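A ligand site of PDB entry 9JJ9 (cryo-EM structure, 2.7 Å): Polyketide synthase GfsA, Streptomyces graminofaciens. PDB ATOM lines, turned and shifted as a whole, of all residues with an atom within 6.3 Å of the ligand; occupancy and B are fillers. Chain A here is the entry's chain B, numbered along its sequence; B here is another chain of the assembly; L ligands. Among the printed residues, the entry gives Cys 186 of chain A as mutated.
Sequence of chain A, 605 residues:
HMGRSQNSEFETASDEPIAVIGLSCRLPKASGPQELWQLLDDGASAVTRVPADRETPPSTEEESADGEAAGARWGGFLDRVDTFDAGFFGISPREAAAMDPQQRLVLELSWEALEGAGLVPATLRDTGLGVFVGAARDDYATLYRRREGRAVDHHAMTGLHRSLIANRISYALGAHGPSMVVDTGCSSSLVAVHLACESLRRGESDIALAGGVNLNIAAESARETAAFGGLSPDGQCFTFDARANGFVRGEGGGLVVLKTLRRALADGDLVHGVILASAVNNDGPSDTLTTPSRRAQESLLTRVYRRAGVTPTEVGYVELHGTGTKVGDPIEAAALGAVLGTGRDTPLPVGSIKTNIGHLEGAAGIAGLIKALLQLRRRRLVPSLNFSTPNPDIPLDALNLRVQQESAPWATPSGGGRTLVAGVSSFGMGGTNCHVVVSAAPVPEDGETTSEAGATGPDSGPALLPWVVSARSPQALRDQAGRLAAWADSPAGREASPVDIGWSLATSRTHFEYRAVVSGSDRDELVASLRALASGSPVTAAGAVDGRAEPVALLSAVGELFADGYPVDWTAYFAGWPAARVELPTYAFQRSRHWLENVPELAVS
A phosphorus (P1) of the ligand is covalently linked to the side-chain hydroxyl (OG) of Ser 49 of chain B (1.6 Å). C13 of the ligand is covalently linked to SG of Cys 186, at 1.8 Å. The side-chain hydroxyl (OG1) of Thr 291 lies within hydrogen-bond range of an oxygen (O1) of the ligand, 3.2 Å away.
ND1 of His 359 is in hydrogen-bond range of N of Glu 361, at 3.2 Å. The side-chain hydroxyl (OG1) of Thr 323 sits at hydrogen-bond distance from the side-chain hydroxyl (OG1) of Thr 325 (3.2 Å). The backbone NH of Thr 325 is in hydrogen-bond range of the side-chain carboxylate of Asp 329, at 3.4 Å.
Merely in contact with the ligand: Met 429, Val 327, His 359, Thr 325, Thr 290, Leu 50 of chain B, Thr 323, Gly 328, Phe 228, Glu 361 and Gly 428. Of the 26 residues printed, 14 come within 4 Å of the ligand. The nearest printed residue that does not touch the ligand is Phe 247 (4.1 Å).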
ATOM      1  N   GLY A 185      12.994 -20.788   9.077  1.00  0.00           N
ATOM      2  CA  GLY A 185      12.598 -20.449   7.728  1.00  0.00           C
ATOM      3  C   GLY A 185      11.380 -19.553   7.686  1.00  0.00           C
ATOM      4  O   GLY A 185      11.394 -18.453   8.244  1.00  0.00           O
ATOM      5  N   CYS A 186      10.316 -20.007   7.026  1.00  0.00           N
ATOM      6  CA  CYS A 186       9.081 -19.258   6.926  1.00  0.00           C
ATOM      7  C   CYS A 186       8.184 -19.436   8.140  1.00  0.00           C
ATOM      8  O   CYS A 186       7.153 -18.750   8.241  1.00  0.00           O
ATOM      9  CB  CYS A 186       8.315 -19.676   5.664  1.00  0.00           C
ATOM     10  SG  CYS A 186       9.332 -19.751   4.166  1.00  0.00           S
ATOM     11  N   PHE A 228      15.967 -18.882  -8.229  1.00  0.00           N
ATOM     12  CA  PHE A 228      15.305 -20.081  -7.709  1.00  0.00           C
ATOM     13  C   PHE A 228      14.047 -20.412  -8.500  1.00  0.00           C
ATOM     14  O   PHE A 228      13.754 -21.578  -8.766  1.00  0.00           O
ATOM     15  CB  PHE A 228      14.983 -19.905  -6.222  1.00  0.00           C
ATOM     16  CG  PHE A 228      14.428 -21.126  -5.566  1.00  0.00           C
ATOM     17  CD1 PHE A 228      13.069 -21.253  -5.324  1.00  0.00           C
ATOM     18  CD2 PHE A 228      15.265 -22.169  -5.193  1.00  0.00           C
ATOM     19  CE1 PHE A 228      12.554 -22.378  -4.718  1.00  0.00           C
ATOM     20  CE2 PHE A 228      14.753 -23.303  -4.577  1.00  0.00           C
ATOM     21  CZ  PHE A 228      13.399 -23.409  -4.346  1.00  0.00           C
ATOM     22  N   GLY A 229      13.288 -19.386  -8.880  1.00  0.00           N
ATOM     23  CA  GLY A 229      12.072 -19.591  -9.647  1.00  0.00           C
ATOM     24  C   GLY A 229      10.830 -19.656  -8.792  1.00  0.00           C
ATOM     25  O   GLY A 229      10.009 -20.574  -8.935  1.00  0.00           O
ATOM     26  N   PHE A 247       4.934 -16.013  -5.319  1.00  0.00           N
ATOM     27  CA  PHE A 247       4.692 -15.072  -4.232  1.00  0.00           C
ATOM     28  C   PHE A 247       5.436 -13.763  -4.511  1.00  0.00           C
ATOM     29  O   PHE A 247       6.164 -13.633  -5.494  1.00  0.00           O
ATOM     30  CB  PHE A 247       5.111 -15.662  -2.890  1.00  0.00           C
ATOM     31  CG  PHE A 247       6.517 -16.200  -2.867  1.00  0.00           C
ATOM     32  CD1 PHE A 247       7.585 -15.368  -2.575  1.00  0.00           C
ATOM     33  CD2 PHE A 247       6.769 -17.530  -3.138  1.00  0.00           C
ATOM     34  CE1 PHE A 247       8.883 -15.861  -2.553  1.00  0.00           C
ATOM     35  CE2 PHE A 247       8.058 -18.034  -3.114  1.00  0.00           C
ATOM     36  CZ  PHE A 247       9.112 -17.185  -2.822  1.00  0.00           C
ATOM     37  N   ASP A 287       8.164 -36.163  -0.842  1.00  0.00           N
ATOM     38  CA  ASP A 287       8.639 -36.391  -2.203  1.00  0.00           C
ATOM     39  C   ASP A 287       9.912 -35.615  -2.483  1.00  0.00           C
ATOM     40  O   ASP A 287      10.836 -36.120  -3.127  1.00  0.00           O
ATOM     41  CB  ASP A 287       7.549 -36.032  -3.205  1.00  0.00           C
ATOM     42  CG  ASP A 287       7.971 -36.259  -4.647  1.00  0.00           C
ATOM     43  OD1 ASP A 287       8.416 -37.381  -4.966  1.00  0.00           O
ATOM     44  OD2 ASP A 287       7.873 -35.315  -5.449  1.00  0.00           O
ATOM     45  N   THR A 288       9.981 -34.363  -2.017  1.00  0.00           N
ATOM     46  CA  THR A 288      11.128 -33.510  -2.235  1.00  0.00           C
ATOM     47  C   THR A 288      11.357 -32.680  -0.982  1.00  0.00           C
ATOM     48  O   THR A 288      10.413 -32.317  -0.286  1.00  0.00           O
ATOM     49  CB  THR A 288      10.927 -32.621  -3.483  1.00  0.00           C
ATOM     50  OG1 THR A 288      11.172 -33.395  -4.663  1.00  0.00           O
ATOM     51  CG2 THR A 288      11.858 -31.416  -3.489  1.00  0.00           C
ATOM     52  N   THR A 290      12.042 -29.685  -0.618  1.00  0.00           N
ATOM     53  CA  THR A 290      11.307 -28.430  -0.704  1.00  0.00           C
ATOM     54  C   THR A 290       9.800 -28.664  -0.750  1.00  0.00           C
ATOM     55  O   THR A 290       9.038 -27.896  -0.145  1.00  0.00           O
ATOM     56  CB  THR A 290      11.764 -27.642  -1.930  1.00  0.00           C
ATOM     57  OG1 THR A 290      13.110 -27.191  -1.738  1.00  0.00           O
ATOM     58  CG2 THR A 290      10.866 -26.421  -2.159  1.00  0.00           C
ATOM     59  N   THR A 291       9.357 -29.703  -1.443  1.00  0.00           N
ATOM     60  CA  THR A 291       7.932 -29.964  -1.581  1.00  0.00           C
ATOM     61  C   THR A 291       7.332 -30.354  -0.226  1.00  0.00           C
ATOM     62  O   THR A 291       7.840 -31.262   0.437  1.00  0.00           O
ATOM     63  CB  THR A 291       7.700 -31.074  -2.602  1.00  0.00           C
ATOM     64  OG1 THR A 291       7.955 -30.578  -3.918  1.00  0.00           O
ATOM     65  CG2 THR A 291       6.258 -31.576  -2.536  1.00  0.00           C
ATOM     66  N   PRO A 292       6.255 -29.694   0.199  1.00  0.00           N
ATOM     67  CA  PRO A 292       5.645 -30.042   1.489  1.00  0.00           C
ATOM     68  C   PRO A 292       4.870 -31.346   1.415  1.00  0.00           C
ATOM     69  O   PRO A 292       4.649 -31.919   0.348  1.00  0.00           O
ATOM     70  CB  PRO A 292       4.721 -28.852   1.777  1.00  0.00           C
ATOM     71  CG  PRO A 292       4.369 -28.339   0.426  1.00  0.00           C
ATOM     72  CD  PRO A 292       5.579 -28.559  -0.441  1.00  0.00           C
ATOM     73  N   HIS A 321      -1.496 -20.245   5.152  1.00  0.00           N
ATOM     74  CA  HIS A 321      -0.093 -20.025   4.846  1.00  0.00           C
ATOM     75  C   HIS A 321       0.168 -20.003   3.347  1.00  0.00           C
ATOM     76  O   HIS A 321       1.333 -20.087   2.930  1.00  0.00           O
ATOM     77  CB  HIS A 321       0.768 -21.091   5.530  1.00  0.00           C
ATOM     78  CG  HIS A 321       2.234 -20.793   5.527  1.00  0.00           C
ATOM     79  ND1 HIS A 321       2.785 -19.768   6.266  1.00  0.00           N
ATOM     80  CD2 HIS A 321       3.269 -21.387   4.873  1.00  0.00           C
ATOM     81  CE1 HIS A 321       4.092 -19.739   6.065  1.00  0.00           C
ATOM     82  NE2 HIS A 321       4.402 -20.709   5.234  1.00  0.00           N
ATOM     83  N   THR A 323       1.120 -19.375  -0.338  1.00  0.00           N
ATOM     84  CA  THR A 323       2.127 -18.525  -0.956  1.00  0.00           C
ATOM     85  C   THR A 323       1.781 -18.158  -2.390  1.00  0.00           C
ATOM     86  O   THR A 323       2.643 -17.663  -3.122  1.00  0.00           O
ATOM     87  CB  THR A 323       3.498 -19.206  -0.907  1.00  0.00           C
ATOM     88  OG1 THR A 323       3.496 -20.340  -1.767  1.00  0.00           O
ATOM     89  CG2 THR A 323       3.813 -19.655   0.509  1.00  0.00           C
ATOM     90  N   THR A 325       1.019 -20.292  -4.855  1.00  0.00           N
ATOM     91  CA  THR A 325       1.617 -21.276  -5.753  1.00  0.00           C
ATOM     92  C   THR A 325       0.681 -22.465  -5.895  1.00  0.00           C
ATOM     93  O   THR A 325       0.002 -22.856  -4.934  1.00  0.00           O
ATOM     94  CB  THR A 325       2.979 -21.751  -5.240  1.00  0.00           C
ATOM     95  OG1 THR A 325       2.810 -22.461  -4.000  1.00  0.00           O
ATOM     96  CG2 THR A 325       3.918 -20.564  -5.015  1.00  0.00           C
ATOM     97  N   VAL A 327       1.296 -25.500  -6.047  1.00  0.00           N
ATOM     98  CA  VAL A 327       1.886 -26.734  -5.531  1.00  0.00           C
ATOM     99  C   VAL A 327       1.472 -26.984  -4.089  1.00  0.00           C
ATOM    100  O   VAL A 327       0.846 -27.996  -3.779  1.00  0.00           O
ATOM    101  CB  VAL A 327       3.429 -26.709  -5.680  1.00  0.00           C
ATOM    102  CG1 VAL A 327       4.044 -27.910  -4.986  1.00  0.00           C
ATOM    103  CG2 VAL A 327       3.820 -26.674  -7.142  1.00  0.00           C
ATOM    104  N   GLY A 328       1.818 -26.066  -3.181  1.00  0.00           N
ATOM    105  CA  GLY A 328       1.486 -26.244  -1.774  1.00  0.00           C
ATOM    106  C   GLY A 328       0.060 -25.872  -1.409  1.00  0.00           C
ATOM    107  O   GLY A 328      -0.458 -26.379  -0.410  1.00  0.00           O
ATOM    108  N   ASP A 329      -0.568 -24.988  -2.178  1.00  0.00           N
ATOM    109  CA  ASP A 329      -1.951 -24.600  -1.897  1.00  0.00           C
ATOM    110  C   ASP A 329      -2.920 -25.762  -1.978  1.00  0.00           C
ATOM    111  O   ASP A 329      -3.759 -25.904  -1.073  1.00  0.00           O
ATOM    112  CB  ASP A 329      -2.362 -23.456  -2.818  1.00  0.00           C
ATOM    113  CG  ASP A 329      -1.750 -22.129  -2.423  1.00  0.00           C
ATOM    114  OD1 ASP A 329      -1.190 -22.046  -1.309  1.00  0.00           O
ATOM    115  OD2 ASP A 329      -1.838 -21.166  -3.220  1.00  0.00           O
ATOM    116  N   HIS A 359       4.516 -12.025   0.848  1.00  0.00           N
ATOM    117  CA  HIS A 359       5.236 -12.978   1.686  1.00  0.00           C
ATOM    118  C   HIS A 359       6.447 -12.302   2.314  1.00  0.00           C
ATOM    119  O   HIS A 359       7.202 -11.599   1.639  1.00  0.00           O
ATOM    120  CB  HIS A 359       5.669 -14.187   0.862  1.00  0.00           C
ATOM    121  CG  HIS A 359       5.757 -15.454   1.659  1.00  0.00           C
ATOM    122  ND1 HIS A 359       6.273 -15.496   2.942  1.00  0.00           N
ATOM    123  CD2 HIS A 359       5.389 -16.727   1.356  1.00  0.00           C
ATOM    124  CE1 HIS A 359       6.221 -16.738   3.384  1.00  0.00           C
ATOM    125  NE2 HIS A 359       5.697 -17.503   2.446  1.00  0.00           N
ATOM    126  N   GLU A 361       8.491 -14.259   4.850  1.00  0.00           N
ATOM    127  CA  GLU A 361       9.416 -15.378   5.008  1.00  0.00           C
ATOM    128  C   GLU A 361      10.226 -15.280   6.293  1.00  0.00           C
ATOM    129  O   GLU A 361      11.050 -16.163   6.571  1.00  0.00           O
ATOM    130  CB  GLU A 361      10.344 -15.481   3.788  1.00  0.00           C
ATOM    131  CG  GLU A 361       9.621 -15.738   2.474  1.00  0.00           C
ATOM    132  CD  GLU A 361      10.367 -15.182   1.287  1.00  0.00           C
ATOM    133  OE1 GLU A 361      10.369 -13.953   1.106  1.00  0.00           O
ATOM    134  OE2 GLU A 361      10.946 -15.990   0.520  1.00  0.00           O
ATOM    135  N   PHE A 427       4.201 -22.826   7.486  1.00  0.00           N
ATOM    136  CA  PHE A 427       5.011 -23.921   6.974  1.00  0.00           C
ATOM    137  C   PHE A 427       6.352 -23.381   6.506  1.00  0.00           C
ATOM    138  O   PHE A 427       6.411 -22.454   5.687  1.00  0.00           O
ATOM    139  CB  PHE A 427       4.292 -24.622   5.815  1.00  0.00           C
ATOM    140  CG  PHE A 427       2.857 -24.965   6.106  1.00  0.00           C
ATOM    141  CD1 PHE A 427       2.498 -25.513   7.327  1.00  0.00           C
ATOM    142  CD2 PHE A 427       1.870 -24.752   5.151  1.00  0.00           C
ATOM    143  CE1 PHE A 427       1.175 -25.830   7.594  1.00  0.00           C
ATOM    144  CE2 PHE A 427       0.555 -25.057   5.417  1.00  0.00           C
ATOM    145  CZ  PHE A 427       0.210 -25.606   6.634  1.00  0.00           C
ATOM    146  N   GLY A 428       7.434 -23.971   7.016  1.00  0.00           N
ATOM    147  CA  GLY A 428       8.759 -23.540   6.639  1.00  0.00           C
ATOM    148  C   GLY A 428       9.184 -24.090   5.284  1.00  0.00           C
ATOM    149  O   GLY A 428       8.609 -25.039   4.753  1.00  0.00           O
ATOM    150  N   MET A 429      10.212 -23.459   4.717  1.00  0.00           N
ATOM    151  CA  MET A 429      10.753 -23.908   3.441  1.00  0.00           C
ATOM    152  C   MET A 429      11.367 -25.302   3.560  1.00  0.00           C
ATOM    153  O   MET A 429      11.205 -26.135   2.661  1.00  0.00           O
ATOM    154  CB  MET A 429      11.778 -22.910   2.910  1.00  0.00           C
ATOM    155  CG  MET A 429      12.400 -22.036   3.988  1.00  0.00           C
ATOM    156  SD  MET A 429      13.504 -20.782   3.309  1.00  0.00           S
ATOM    157  CE  MET A 429      14.830 -21.813   2.684  1.00  0.00           C
ATOM    158  N   GLY A 430      12.064 -25.568   4.666  1.00  0.00           N
ATOM    159  CA  GLY A 430      12.687 -26.861   4.853  1.00  0.00           C
ATOM    160  C   GLY A 430      11.713 -27.988   5.151  1.00  0.00           C
ATOM    161  O   GLY A 430      12.050 -29.150   4.920  1.00  0.00           O
ATOM    162  N   ASP B  48      14.913 -33.777  -8.894  1.00  0.00           N
ATOM    163  CA  ASP B  48      13.768 -33.032  -8.386  1.00  0.00           C
ATOM    164  C   ASP B  48      12.888 -32.604  -9.562  1.00  0.00           C
ATOM    165  O   ASP B  48      13.086 -33.041 -10.701  1.00  0.00           O
ATOM    166  CB  ASP B  48      14.239 -31.846  -7.542  1.00  0.00           C
ATOM    167  CG  ASP B  48      15.276 -30.997  -8.235  1.00  0.00           C
ATOM    168  OD1 ASP B  48      15.454 -31.142  -9.466  1.00  0.00           O
ATOM    169  OD2 ASP B  48      15.926 -30.175  -7.557  1.00  0.00           O
ATOM    170  N   SER B  49      11.895 -31.758  -9.281  1.00  0.00           N
ATOM    171  CA  SER B  49      10.980 -31.321 -10.326  1.00  0.00           C
ATOM    172  C   SER B  49      11.712 -30.511 -11.400  1.00  0.00           C
ATOM    173  O   SER B  49      11.436 -30.665 -12.591  1.00  0.00           O
ATOM    174  CB  SER B  49       9.845 -30.499  -9.723  1.00  0.00           C
ATOM    175  OG  SER B  49       9.474 -31.010  -8.446  1.00  0.00           O
ATOM    176  N   LEU B  50      12.640 -29.647 -10.985  1.00  0.00           N
ATOM    177  CA  LEU B  50      13.325 -28.780 -11.950  1.00  0.00           C
ATOM    178  C   LEU B  50      14.161 -29.602 -12.919  1.00  0.00           C
ATOM    179  O   LEU B  50      14.092 -29.395 -14.140  1.00  0.00           O
ATOM    180  CB  LEU B  50      14.209 -27.775 -11.207  1.00  0.00           C
ATOM    181  CG  LEU B  50      13.547 -26.619 -10.448  1.00  0.00           C
ATOM    182  CD1 LEU B  50      12.880 -27.082  -9.159  1.00  0.00           C
ATOM    183  CD2 LEU B  50      14.560 -25.517 -10.161  1.00  0.00           C
ATOM    184  N   VAL B  53      11.870 -31.567 -15.317  1.00  0.00           N
ATOM    185  CA  VAL B  53      11.334 -30.728 -16.389  1.00  0.00           C
ATOM    186  C   VAL B  53      12.420 -30.401 -17.414  1.00  0.00           C
ATOM    187  O   VAL B  53      12.180 -30.445 -18.623  1.00  0.00           O
ATOM    188  CB  VAL B  53      10.703 -29.446 -15.796  1.00  0.00           C
ATOM    189  CG1 VAL B  53      10.362 -28.457 -16.910  1.00  0.00           C
ATOM    190  CG2 VAL B  53       9.471 -29.791 -14.991  1.00  0.00           C
HETATM  191  O1  LIG L   1       8.425 -30.433  -7.035  1.00  0.00           O
HETATM  192  P1  LIG L   1       8.586 -29.725  -8.352  1.00  0.00           P
HETATM  193  O2  LIG L   1       7.370 -29.972  -9.214  1.00  0.00           O
HETATM  194  O3  LIG L   1       8.694 -28.145  -8.076  1.00  0.00           O
HETATM  195  C1  LIG L   1       9.718 -27.617  -7.234  1.00  0.00           C
HETATM  196  C2  LIG L   1       9.508 -26.112  -7.079  1.00  0.00           C
HETATM  197  C3  LIG L   1       9.643 -25.459  -8.448  1.00  0.00           C
HETATM  198  C4  LIG L   1      10.555 -25.523  -6.141  1.00  0.00           C
HETATM  199  C5  LIG L   1       8.099 -25.822  -6.570  1.00  0.00           C
HETATM  200  O4  LIG L   1       7.159 -26.592  -7.340  1.00  0.00           O
HETATM  201  C6  LIG L   1       7.880 -26.127  -5.111  1.00  0.00           C
HETATM  202  O5  LIG L   1       8.431 -27.053  -4.523  1.00  0.00           O
HETATM  203  N1  LIG L   1       7.020 -25.329  -4.494  1.00  0.00           N
HETATM  204  C7  LIG L   1       6.611 -25.375  -3.094  1.00  0.00           C
HETATM  205  C8  LIG L   1       5.355 -24.514  -3.032  1.00  0.00           C
HETATM  206  C9  LIG L   1       5.318 -23.777  -1.716  1.00  0.00           C
HETATM  207  O6  LIG L   1       4.425 -23.986  -0.905  1.00  0.00           O
HETATM  208  N2  LIG L   1       6.306 -22.902  -1.500  1.00  0.00           N
HETATM  209  C10 LIG L   1       6.503 -22.059  -0.332  1.00  0.00           C
HETATM  210  C11 LIG L   1       7.777 -21.277  -0.636  1.00  0.00           C
HETATM  211  N3  LIG L   1       7.952 -20.372   0.496  1.00  0.00           N
HETATM  212  C12 LIG L   1       8.324 -20.680   1.734  1.00  0.00           C
HETATM  213  O7  LIG L   1       8.572 -21.820   2.075  1.00  0.00           O
HETATM  214  C13 LIG L   1       8.418 -19.522   2.678  1.00  0.00           C
